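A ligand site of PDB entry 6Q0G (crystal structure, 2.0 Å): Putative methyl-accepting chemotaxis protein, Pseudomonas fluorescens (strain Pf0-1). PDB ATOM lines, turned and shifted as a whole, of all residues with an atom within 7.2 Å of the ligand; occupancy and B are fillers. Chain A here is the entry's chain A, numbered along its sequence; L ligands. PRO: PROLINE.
OD2 of Asp 146 is in salt-bridge range of N of the ligand. The indole nitrogen (NE1) of Trp 101 lies within hydrogen-bond range of an oxygen (O) of the ligand, at 2.8 Å. An oxygen (O) of the ligand is in salt-bridge range of the guanidinium group (NE) of Arg 99, at 2.6 Å. N of Ala 120 lies within hydrogen-bond range of OXT of the ligand. A nitrogen (N) of the ligand lies within salt-bridge range of the side-chain carboxylate of Asp 119 (2.9 Å).
O of Ile 118 sits at hydrogen-bond distance from NH2 of Arg 99 (2.8 Å). OD2 of Asp 119 sits at hydrogen-bond distance from OG1 of Thr 122 (2.5 Å). O of Gly 144 is in hydrogen-bond range of N of Tyr 74, at 3.0 Å. The side-chain carboxylate (OD1) of Asp 119 lies within hydrogen-bond range of the backbone NH (N) of Ala 121, 3.0 Å away. The backbone NH (N) of Asp 146 is in hydrogen-bond range of the backbone carbonyl oxygen (O) of Ala 72 (3.1 Å). The backbone carbonyl oxygen (O) of Tyr 117 sits at hydrogen-bond distance from the backbone NH (N) of Ile 126 (2.9 Å). O of Gln 124 sits at hydrogen-bond distance from N of Asp 119, 2.8 Å away. The side-chain hydroxyl (OG) of Ser 128 sits at hydrogen-bond distance from the side-chain hydroxyl (OH) of Tyr 117.
Residues that only touch the ligand: Tyr 117 (3.3 Å), Phe 82 (3.5 Å), Tyr 74 (3.5 Å), Met 90 (3.6 Å), Ile 84 (3.7 Å), Phe 94 (3.8 Å) and Ile 126 (3.9 Å). The nearest printed residue that does not touch the ligand is Ala 121 (4.1 Å).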
ATOM      1  N   ALA A  72      -5.193 -27.166   5.390  1.00  0.00           N
ATOM      2  CA  ALA A  72      -6.624 -26.988   5.475  1.00  0.00           C
ATOM      3  C   ALA A  72      -6.865 -25.554   5.067  1.00  0.00           C
ATOM      4  O   ALA A  72      -5.941 -24.726   5.159  1.00  0.00           O
ATOM      5  CB  ALA A  72      -7.153 -27.208   6.907  1.00  0.00           C
ATOM      6  N   SER A  73      -8.092 -25.268   4.667  1.00  0.00           N
ATOM      7  CA  SER A  73      -8.533 -23.897   4.464  1.00  0.00           C
ATOM      8  C   SER A  73      -9.882 -23.758   5.133  1.00  0.00           C
ATOM      9  O   SER A  73     -10.563 -24.764   5.402  1.00  0.00           O
ATOM     10  CB  SER A  73      -8.583 -23.514   2.961  1.00  0.00           C
ATOM     11  OG  SER A  73      -9.367 -24.463   2.287  1.00  0.00           O
ATOM     12  N   TYR A  74     -10.274 -22.521   5.412  1.00  0.00           N
ATOM     13  CA  TYR A  74     -11.362 -22.342   6.341  1.00  0.00           C
ATOM     14  C   TYR A  74     -11.909 -20.931   6.220  1.00  0.00           C
ATOM     15  O   TYR A  74     -11.264 -20.033   5.687  1.00  0.00           O
ATOM     16  CB  TYR A  74     -10.911 -22.601   7.806  1.00  0.00           C
ATOM     17  CG  TYR A  74      -9.492 -22.105   8.048  1.00  0.00           C
ATOM     18  CD1 TYR A  74      -9.264 -20.756   8.369  1.00  0.00           C
ATOM     19  CD2 TYR A  74      -8.410 -22.939   7.890  1.00  0.00           C
ATOM     20  CE1 TYR A  74      -7.971 -20.264   8.552  1.00  0.00           C
ATOM     21  CE2 TYR A  74      -7.097 -22.446   8.082  1.00  0.00           C
ATOM     22  CZ  TYR A  74      -6.896 -21.101   8.435  1.00  0.00           C
ATOM     23  OH  TYR A  74      -5.622 -20.601   8.630  1.00  0.00           O
ATOM     24  N   PHE A  82     -17.247 -21.049  12.191  1.00  0.00           N
ATOM     25  CA  PHE A  82     -16.005 -21.592  11.642  1.00  0.00           C
ATOM     26  C   PHE A  82     -16.337 -22.806  10.784  1.00  0.00           C
ATOM     27  O   PHE A  82     -17.027 -23.722  11.240  1.00  0.00           O
ATOM     28  CB  PHE A  82     -15.013 -21.961  12.762  1.00  0.00           C
ATOM     29  CG  PHE A  82     -13.628 -22.308  12.251  1.00  0.00           C
ATOM     30  CD1 PHE A  82     -12.867 -21.375  11.568  1.00  0.00           C
ATOM     31  CD2 PHE A  82     -13.083 -23.573  12.459  1.00  0.00           C
ATOM     32  CE1 PHE A  82     -11.582 -21.679  11.098  1.00  0.00           C
ATOM     33  CE2 PHE A  82     -11.824 -23.881  12.032  1.00  0.00           C
ATOM     34  CZ  PHE A  82     -11.065 -22.937  11.330  1.00  0.00           C
ATOM     35  N   ILE A  84     -14.133 -25.505   8.311  1.00  0.00           N
ATOM     36  CA  ILE A  84     -12.785 -25.900   7.921  1.00  0.00           C
ATOM     37  C   ILE A  84     -12.850 -27.171   7.088  1.00  0.00           C
ATOM     38  O   ILE A  84     -13.648 -28.063   7.363  1.00  0.00           O
ATOM     39  CB  ILE A  84     -11.866 -26.050   9.170  1.00  0.00           C
ATOM     40  CG1 ILE A  84     -10.413 -26.086   8.729  1.00  0.00           C
ATOM     41  CG2 ILE A  84     -12.293 -27.237  10.061  1.00  0.00           C
ATOM     42  CD1 ILE A  84      -9.364 -26.203   9.877  1.00  0.00           C
ATOM     43  N   MET A  90     -12.198 -28.941  16.378  1.00  0.00           N
ATOM     44  CA  MET A  90     -11.368 -27.894  16.952  1.00  0.00           C
ATOM     45  C   MET A  90     -11.456 -27.955  18.474  1.00  0.00           C
ATOM     46  O   MET A  90     -12.479 -28.393  19.024  1.00  0.00           O
ATOM     47  CB  MET A  90     -11.832 -26.529  16.470  1.00  0.00           C
ATOM     48  CG  MET A  90     -11.822 -26.428  14.876  1.00  0.00           C
ATOM     49  SD  MET A  90     -10.201 -26.856  14.249  1.00  0.00           S
ATOM     50  CE  MET A  90      -9.359 -25.388  14.663  1.00  0.00           C
ATOM     51  N   PHE A  94     -12.301 -22.915  20.959  1.00  0.00           N
ATOM     52  CA  PHE A  94     -11.587 -22.302  19.852  1.00  0.00           C
ATOM     53  C   PHE A  94     -12.425 -21.173  19.300  1.00  0.00           C
ATOM     54  O   PHE A  94     -13.621 -21.346  19.064  1.00  0.00           O
ATOM     55  CB  PHE A  94     -11.286 -23.347  18.756  1.00  0.00           C
ATOM     56  CG  PHE A  94     -10.830 -22.756  17.430  1.00  0.00           C
ATOM     57  CD1 PHE A  94      -9.500 -22.430  17.219  1.00  0.00           C
ATOM     58  CD2 PHE A  94     -11.723 -22.547  16.413  1.00  0.00           C
ATOM     59  CE1 PHE A  94      -9.072 -21.906  15.992  1.00  0.00           C
ATOM     60  CE2 PHE A  94     -11.307 -22.014  15.178  1.00  0.00           C
ATOM     61  CZ  PHE A  94      -9.984 -21.699  14.988  1.00  0.00           C
ATOM     62  N   ASP A  95     -11.817 -20.015  19.105  1.00  0.00           N
ATOM     63  CA  ASP A  95     -12.518 -18.868  18.522  1.00  0.00           C
ATOM     64  C   ASP A  95     -11.682 -18.365  17.358  1.00  0.00           C
ATOM     65  O   ASP A  95     -10.544 -17.913  17.573  1.00  0.00           O
ATOM     66  CB  ASP A  95     -12.745 -17.776  19.583  1.00  0.00           C
ATOM     67  CG  ASP A  95     -13.601 -16.621  19.074  1.00  0.00           C
ATOM     68  OD1 ASP A  95     -13.793 -16.483  17.852  1.00  0.00           O
ATOM     69  OD2 ASP A  95     -14.083 -15.811  19.892  1.00  0.00           O
ATOM     70  N   PRO A  96     -12.174 -18.452  16.111  1.00  0.00           N
ATOM     71  CA  PRO A  96     -11.343 -17.972  14.987  1.00  0.00           C
ATOM     72  C   PRO A  96     -10.990 -16.504  15.091  1.00  0.00           C
ATOM     73  O   PRO A  96      -9.914 -16.110  14.655  1.00  0.00           O
ATOM     74  CB  PRO A  96     -12.226 -18.252  13.743  1.00  0.00           C
ATOM     75  CG  PRO A  96     -13.673 -18.191  14.275  1.00  0.00           C
ATOM     76  CD  PRO A  96     -13.557 -18.776  15.703  1.00  0.00           C
ATOM     77  N   VAL A  98      -9.888 -14.668  17.401  1.00  0.00           N
ATOM     78  CA  VAL A  98      -8.718 -14.296  18.182  1.00  0.00           C
ATOM     79  C   VAL A  98      -7.432 -14.916  17.625  1.00  0.00           C
ATOM     80  O   VAL A  98      -6.351 -14.688  18.195  1.00  0.00           O
ATOM     81  CB  VAL A  98      -8.924 -14.651  19.659  1.00  0.00           C
ATOM     82  CG1 VAL A  98     -10.314 -14.170  20.087  1.00  0.00           C
ATOM     83  CG2 VAL A  98      -8.720 -16.141  19.947  1.00  0.00           C
ATOM     84  N   ARG A  99      -7.501 -15.596  16.450  1.00  0.00           N
ATOM     85  CA  ARG A  99      -6.346 -16.252  15.853  1.00  0.00           C
ATOM     86  C   ARG A  99      -5.575 -15.257  14.972  1.00  0.00           C
ATOM     87  O   ARG A  99      -6.139 -14.305  14.447  1.00  0.00           O
ATOM     88  CB  ARG A  99      -6.796 -17.464  15.026  1.00  0.00           C
ATOM     89  CG  ARG A  99      -7.609 -18.479  15.869  1.00  0.00           C
ATOM     90  CD  ARG A  99      -6.745 -19.075  16.979  1.00  0.00           C
ATOM     91  NE  ARG A  99      -5.774 -20.057  16.481  1.00  0.00           N
ATOM     92  CZ  ARG A  99      -4.806 -20.567  17.215  1.00  0.00           C
ATOM     93  NH1 ARG A  99      -4.652 -20.188  18.477  1.00  0.00           N
ATOM     94  NH2 ARG A  99      -4.010 -21.487  16.705  1.00  0.00           N
ATOM     95  N   PRO A 100      -4.281 -15.457  14.797  1.00  0.00           N
ATOM     96  CA  PRO A 100      -3.464 -14.412  14.146  1.00  0.00           C
ATOM     97  C   PRO A 100      -3.842 -14.181  12.693  1.00  0.00           C
ATOM     98  O   PRO A 100      -3.701 -13.061  12.186  1.00  0.00           O
ATOM     99  CB  PRO A 100      -2.041 -14.954  14.295  1.00  0.00           C
ATOM    100  CG  PRO A 100      -2.228 -16.440  14.486  1.00  0.00           C
ATOM    101  CD  PRO A 100      -3.492 -16.630  15.211  1.00  0.00           C
ATOM    102  N   TRP A 101      -4.341 -15.203  12.011  1.00  0.00           N
ATOM    103  CA  TRP A 101      -4.742 -15.017  10.619  1.00  0.00           C
ATOM    104  C   TRP A 101      -5.979 -14.146  10.521  1.00  0.00           C
ATOM    105  O   TRP A 101      -6.146 -13.399   9.548  1.00  0.00           O
ATOM    106  CB  TRP A 101      -4.987 -16.378   9.967  1.00  0.00           C
ATOM    107  CG  TRP A 101      -5.977 -17.266  10.712  1.00  0.00           C
ATOM    108  CD1 TRP A 101      -5.674 -18.203  11.612  1.00  0.00           C
ATOM    109  CD2 TRP A 101      -7.416 -17.316  10.544  1.00  0.00           C
ATOM    110  NE1 TRP A 101      -6.816 -18.841  12.032  1.00  0.00           N
ATOM    111  CE2 TRP A 101      -7.887 -18.303  11.400  1.00  0.00           C
ATOM    112  CE3 TRP A 101      -8.321 -16.637   9.714  1.00  0.00           C
ATOM    113  CZ2 TRP A 101      -9.239 -18.651  11.460  1.00  0.00           C
ATOM    114  CZ3 TRP A 101      -9.652 -16.946   9.805  1.00  0.00           C
ATOM    115  CH2 TRP A 101     -10.112 -17.943  10.669  1.00  0.00           C
ATOM    116  N   TYR A 102      -6.884 -14.270  11.488  1.00  0.00           N
ATOM    117  CA  TYR A 102      -8.102 -13.472  11.445  1.00  0.00           C
ATOM    118  C   TYR A 102      -7.780 -12.018  11.763  1.00  0.00           C
ATOM    119  O   TYR A 102      -8.101 -11.109  10.984  1.00  0.00           O
ATOM    120  CB  TYR A 102      -9.098 -14.064  12.437  1.00  0.00           C
ATOM    121  CG  TYR A 102     -10.457 -13.511  12.334  1.00  0.00           C
ATOM    122  CD1 TYR A 102     -10.764 -12.286  12.896  1.00  0.00           C
ATOM    123  CD2 TYR A 102     -11.465 -14.213  11.693  1.00  0.00           C
ATOM    124  CE1 TYR A 102     -12.021 -11.757  12.792  1.00  0.00           C
ATOM    125  CE2 TYR A 102     -12.705 -13.682  11.557  1.00  0.00           C
ATOM    126  CZ  TYR A 102     -12.992 -12.465  12.107  1.00  0.00           C
ATOM    127  OH  TYR A 102     -14.268 -11.947  12.005  1.00  0.00           O
ATOM    128  N   TYR A 117       2.981 -19.940  14.050  1.00  0.00           N
ATOM    129  CA  TYR A 117       2.196 -20.052  15.269  1.00  0.00           C
ATOM    130  C   TYR A 117       1.801 -21.505  15.390  1.00  0.00           C
ATOM    131  O   TYR A 117       2.075 -22.313  14.500  1.00  0.00           O
ATOM    132  CB  TYR A 117       0.992 -19.075  15.264  1.00  0.00           C
ATOM    133  CG  TYR A 117      -0.121 -19.371  14.271  1.00  0.00           C
ATOM    134  CD1 TYR A 117      -0.048 -18.941  12.940  1.00  0.00           C
ATOM    135  CD2 TYR A 117      -1.262 -20.049  14.678  1.00  0.00           C
ATOM    136  CE1 TYR A 117      -1.104 -19.209  12.034  1.00  0.00           C
ATOM    137  CE2 TYR A 117      -2.315 -20.289  13.824  1.00  0.00           C
ATOM    138  CZ  TYR A 117      -2.232 -19.879  12.490  1.00  0.00           C
ATOM    139  OH  TYR A 117      -3.271 -20.160  11.653  1.00  0.00           O
ATOM    140  N   ILE A 118       1.119 -21.825  16.489  1.00  0.00           N
ATOM    141  CA  ILE A 118       0.754 -23.206  16.782  1.00  0.00           C
ATOM    142  C   ILE A 118      -0.651 -23.484  16.258  1.00  0.00           C
ATOM    143  O   ILE A 118      -1.625 -22.881  16.706  1.00  0.00           O
ATOM    144  CB  ILE A 118       0.849 -23.506  18.286  1.00  0.00           C
ATOM    145  CG1 ILE A 118       2.247 -23.155  18.774  1.00  0.00           C
ATOM    146  CG2 ILE A 118       0.533 -24.979  18.499  1.00  0.00           C
ATOM    147  CD1 ILE A 118       2.404 -23.064  20.343  1.00  0.00           C
ATOM    148  N   ASP A 119      -0.730 -24.387  15.283  1.00  0.00           N
ATOM    149  CA  ASP A 119      -2.001 -24.815  14.699  1.00  0.00           C
ATOM    150  C   ASP A 119      -2.933 -25.358  15.769  1.00  0.00           C
ATOM    151  O   ASP A 119      -2.534 -26.222  16.554  1.00  0.00           O
ATOM    152  CB  ASP A 119      -1.712 -25.894  13.664  1.00  0.00           C
ATOM    153  CG  ASP A 119      -2.941 -26.280  12.887  1.00  0.00           C
ATOM    154  OD1 ASP A 119      -3.966 -25.585  12.913  1.00  0.00           O
ATOM    155  OD2 ASP A 119      -2.876 -27.357  12.304  1.00  0.00           O
ATOM    156  N   ALA A 120      -4.158 -24.816  15.814  1.00  0.00           N
ATOM    157  CA  ALA A 120      -5.186 -25.325  16.732  1.00  0.00           C
ATOM    158  C   ALA A 120      -5.707 -26.663  16.287  1.00  0.00           C
ATOM    159  O   ALA A 120      -6.236 -27.410  17.109  1.00  0.00           O
ATOM    160  CB  ALA A 120      -6.352 -24.332  16.845  1.00  0.00           C
ATOM    161  N   ALA A 121      -5.627 -26.967  14.998  1.00  0.00           N
ATOM    162  CA  ALA A 121      -6.044 -28.276  14.495  1.00  0.00           C
ATOM    163  C   ALA A 121      -5.006 -29.342  14.841  1.00  0.00           C
ATOM    164  O   ALA A 121      -5.266 -30.244  15.642  1.00  0.00           O
ATOM    165  CB  ALA A 121      -6.266 -28.223  12.979  1.00  0.00           C
ATOM    166  N   THR A 122      -3.805 -29.242  14.248  1.00  0.00           N
ATOM    167  CA  THR A 122      -2.802 -30.294  14.317  1.00  0.00           C
ATOM    168  C   THR A 122      -1.828 -30.145  15.476  1.00  0.00           C
ATOM    169  O   THR A 122      -1.047 -31.079  15.721  1.00  0.00           O
ATOM    170  CB  THR A 122      -1.953 -30.307  13.046  1.00  0.00           C
ATOM    171  OG1 THR A 122      -1.205 -29.090  13.013  1.00  0.00           O
ATOM    172  CG2 THR A 122      -2.835 -30.397  11.832  1.00  0.00           C
ATOM    173  N   GLN A 124       0.755 -28.628  15.106  1.00  0.00           N
ATOM    174  CA  GLN A 124       2.006 -28.340  14.408  1.00  0.00           C
ATOM    175  C   GLN A 124       2.240 -26.837  14.314  1.00  0.00           C
ATOM    176  O   GLN A 124       1.317 -26.022  14.437  1.00  0.00           O
ATOM    177  CB  GLN A 124       1.989 -28.913  12.983  1.00  0.00           C
ATOM    178  CG  GLN A 124       1.858 -30.398  12.878  1.00  0.00           C
ATOM    179  CD  GLN A 124       1.713 -30.867  11.429  1.00  0.00           C
ATOM    180  OE1 GLN A 124       2.402 -30.396  10.518  1.00  0.00           O
ATOM    181  NE2 GLN A 124       0.808 -31.818  11.228  1.00  0.00           N
ATOM    182  N   ILE A 126       2.794 -23.690  12.044  1.00  0.00           N
ATOM    183  CA  ILE A 126       2.282 -23.373  10.729  1.00  0.00           C
ATOM    184  C   ILE A 126       2.382 -21.879  10.475  1.00  0.00           C
ATOM    185  O   ILE A 126       2.583 -21.077  11.393  1.00  0.00           O
ATOM    186  CB  ILE A 126       0.820 -23.837  10.592  1.00  0.00           C
ATOM    187  CG1 ILE A 126      -0.093 -23.018  11.548  1.00  0.00           C
ATOM    188  CG2 ILE A 126       0.702 -25.353  10.856  1.00  0.00           C
ATOM    189  CD1 ILE A 126      -1.609 -23.193  11.210  1.00  0.00           C
ATOM    190  N   SER A 128      -0.060 -19.083   7.948  1.00  0.00           N
ATOM    191  CA  SER A 128      -1.356 -19.017   7.291  1.00  0.00           C
ATOM    192  C   SER A 128      -1.378 -17.850   6.318  1.00  0.00           C
ATOM    193  O   SER A 128      -0.824 -16.782   6.606  1.00  0.00           O
ATOM    194  CB  SER A 128      -2.482 -18.877   8.342  1.00  0.00           C
ATOM    195  OG  SER A 128      -2.606 -20.052   9.137  1.00  0.00           O
ATOM    196  N   GLY A 144      -8.742 -18.413   5.388  1.00  0.00           N
ATOM    197  CA  GLY A 144      -7.350 -18.709   5.592  1.00  0.00           C
ATOM    198  C   GLY A 144      -6.964 -20.052   5.047  1.00  0.00           C
ATOM    199  O   GLY A 144      -7.803 -20.949   4.833  1.00  0.00           O
ATOM    200  N   GLY A 145      -5.685 -20.166   4.758  1.00  0.00           N
ATOM    201  CA  GLY A 145      -5.095 -21.438   4.419  1.00  0.00           C
ATOM    202  C   GLY A 145      -3.784 -21.638   5.149  1.00  0.00           C
ATOM    203  O   GLY A 145      -2.964 -20.727   5.264  1.00  0.00           O
ATOM    204  N   ASP A 146      -3.531 -22.877   5.485  1.00  0.00           N
ATOM    205  CA  ASP A 146      -2.422 -23.244   6.324  1.00  0.00           C
ATOM    206  C   ASP A 146      -1.328 -23.973   5.557  1.00  0.00           C
ATOM    207  O   ASP A 146      -1.620 -24.889   4.781  1.00  0.00           O
ATOM    208  CB  ASP A 146      -2.885 -24.156   7.453  1.00  0.00           C
ATOM    209  CG  ASP A 146      -3.725 -23.447   8.488  1.00  0.00           C
ATOM    210  OD1 ASP A 146      -3.723 -22.198   8.562  1.00  0.00           O
ATOM    211  OD2 ASP A 146      -4.372 -24.158   9.252  1.00  0.00           O
HETATM  212  N   PRO L   1      -5.479 -23.421  11.649  1.00  0.00           N
HETATM  213  CA  PRO L   1      -5.954 -22.071  11.981  1.00  0.00           C
HETATM  214  C   PRO L   1      -5.650 -21.735  13.439  1.00  0.00           C
HETATM  215  O   PRO L   1      -6.098 -20.716  13.963  1.00  0.00           O
HETATM  216  CB  PRO L   1      -7.447 -22.160  11.746  1.00  0.00           C
HETATM  217  CG  PRO L   1      -7.748 -23.559  12.062  1.00  0.00           C
HETATM  218  CD  PRO L   1      -6.606 -24.371  11.568  1.00  0.00           C
HETATM  219  OXT PRO L   1      -4.918 -22.502  14.059  1.00  0.00           O
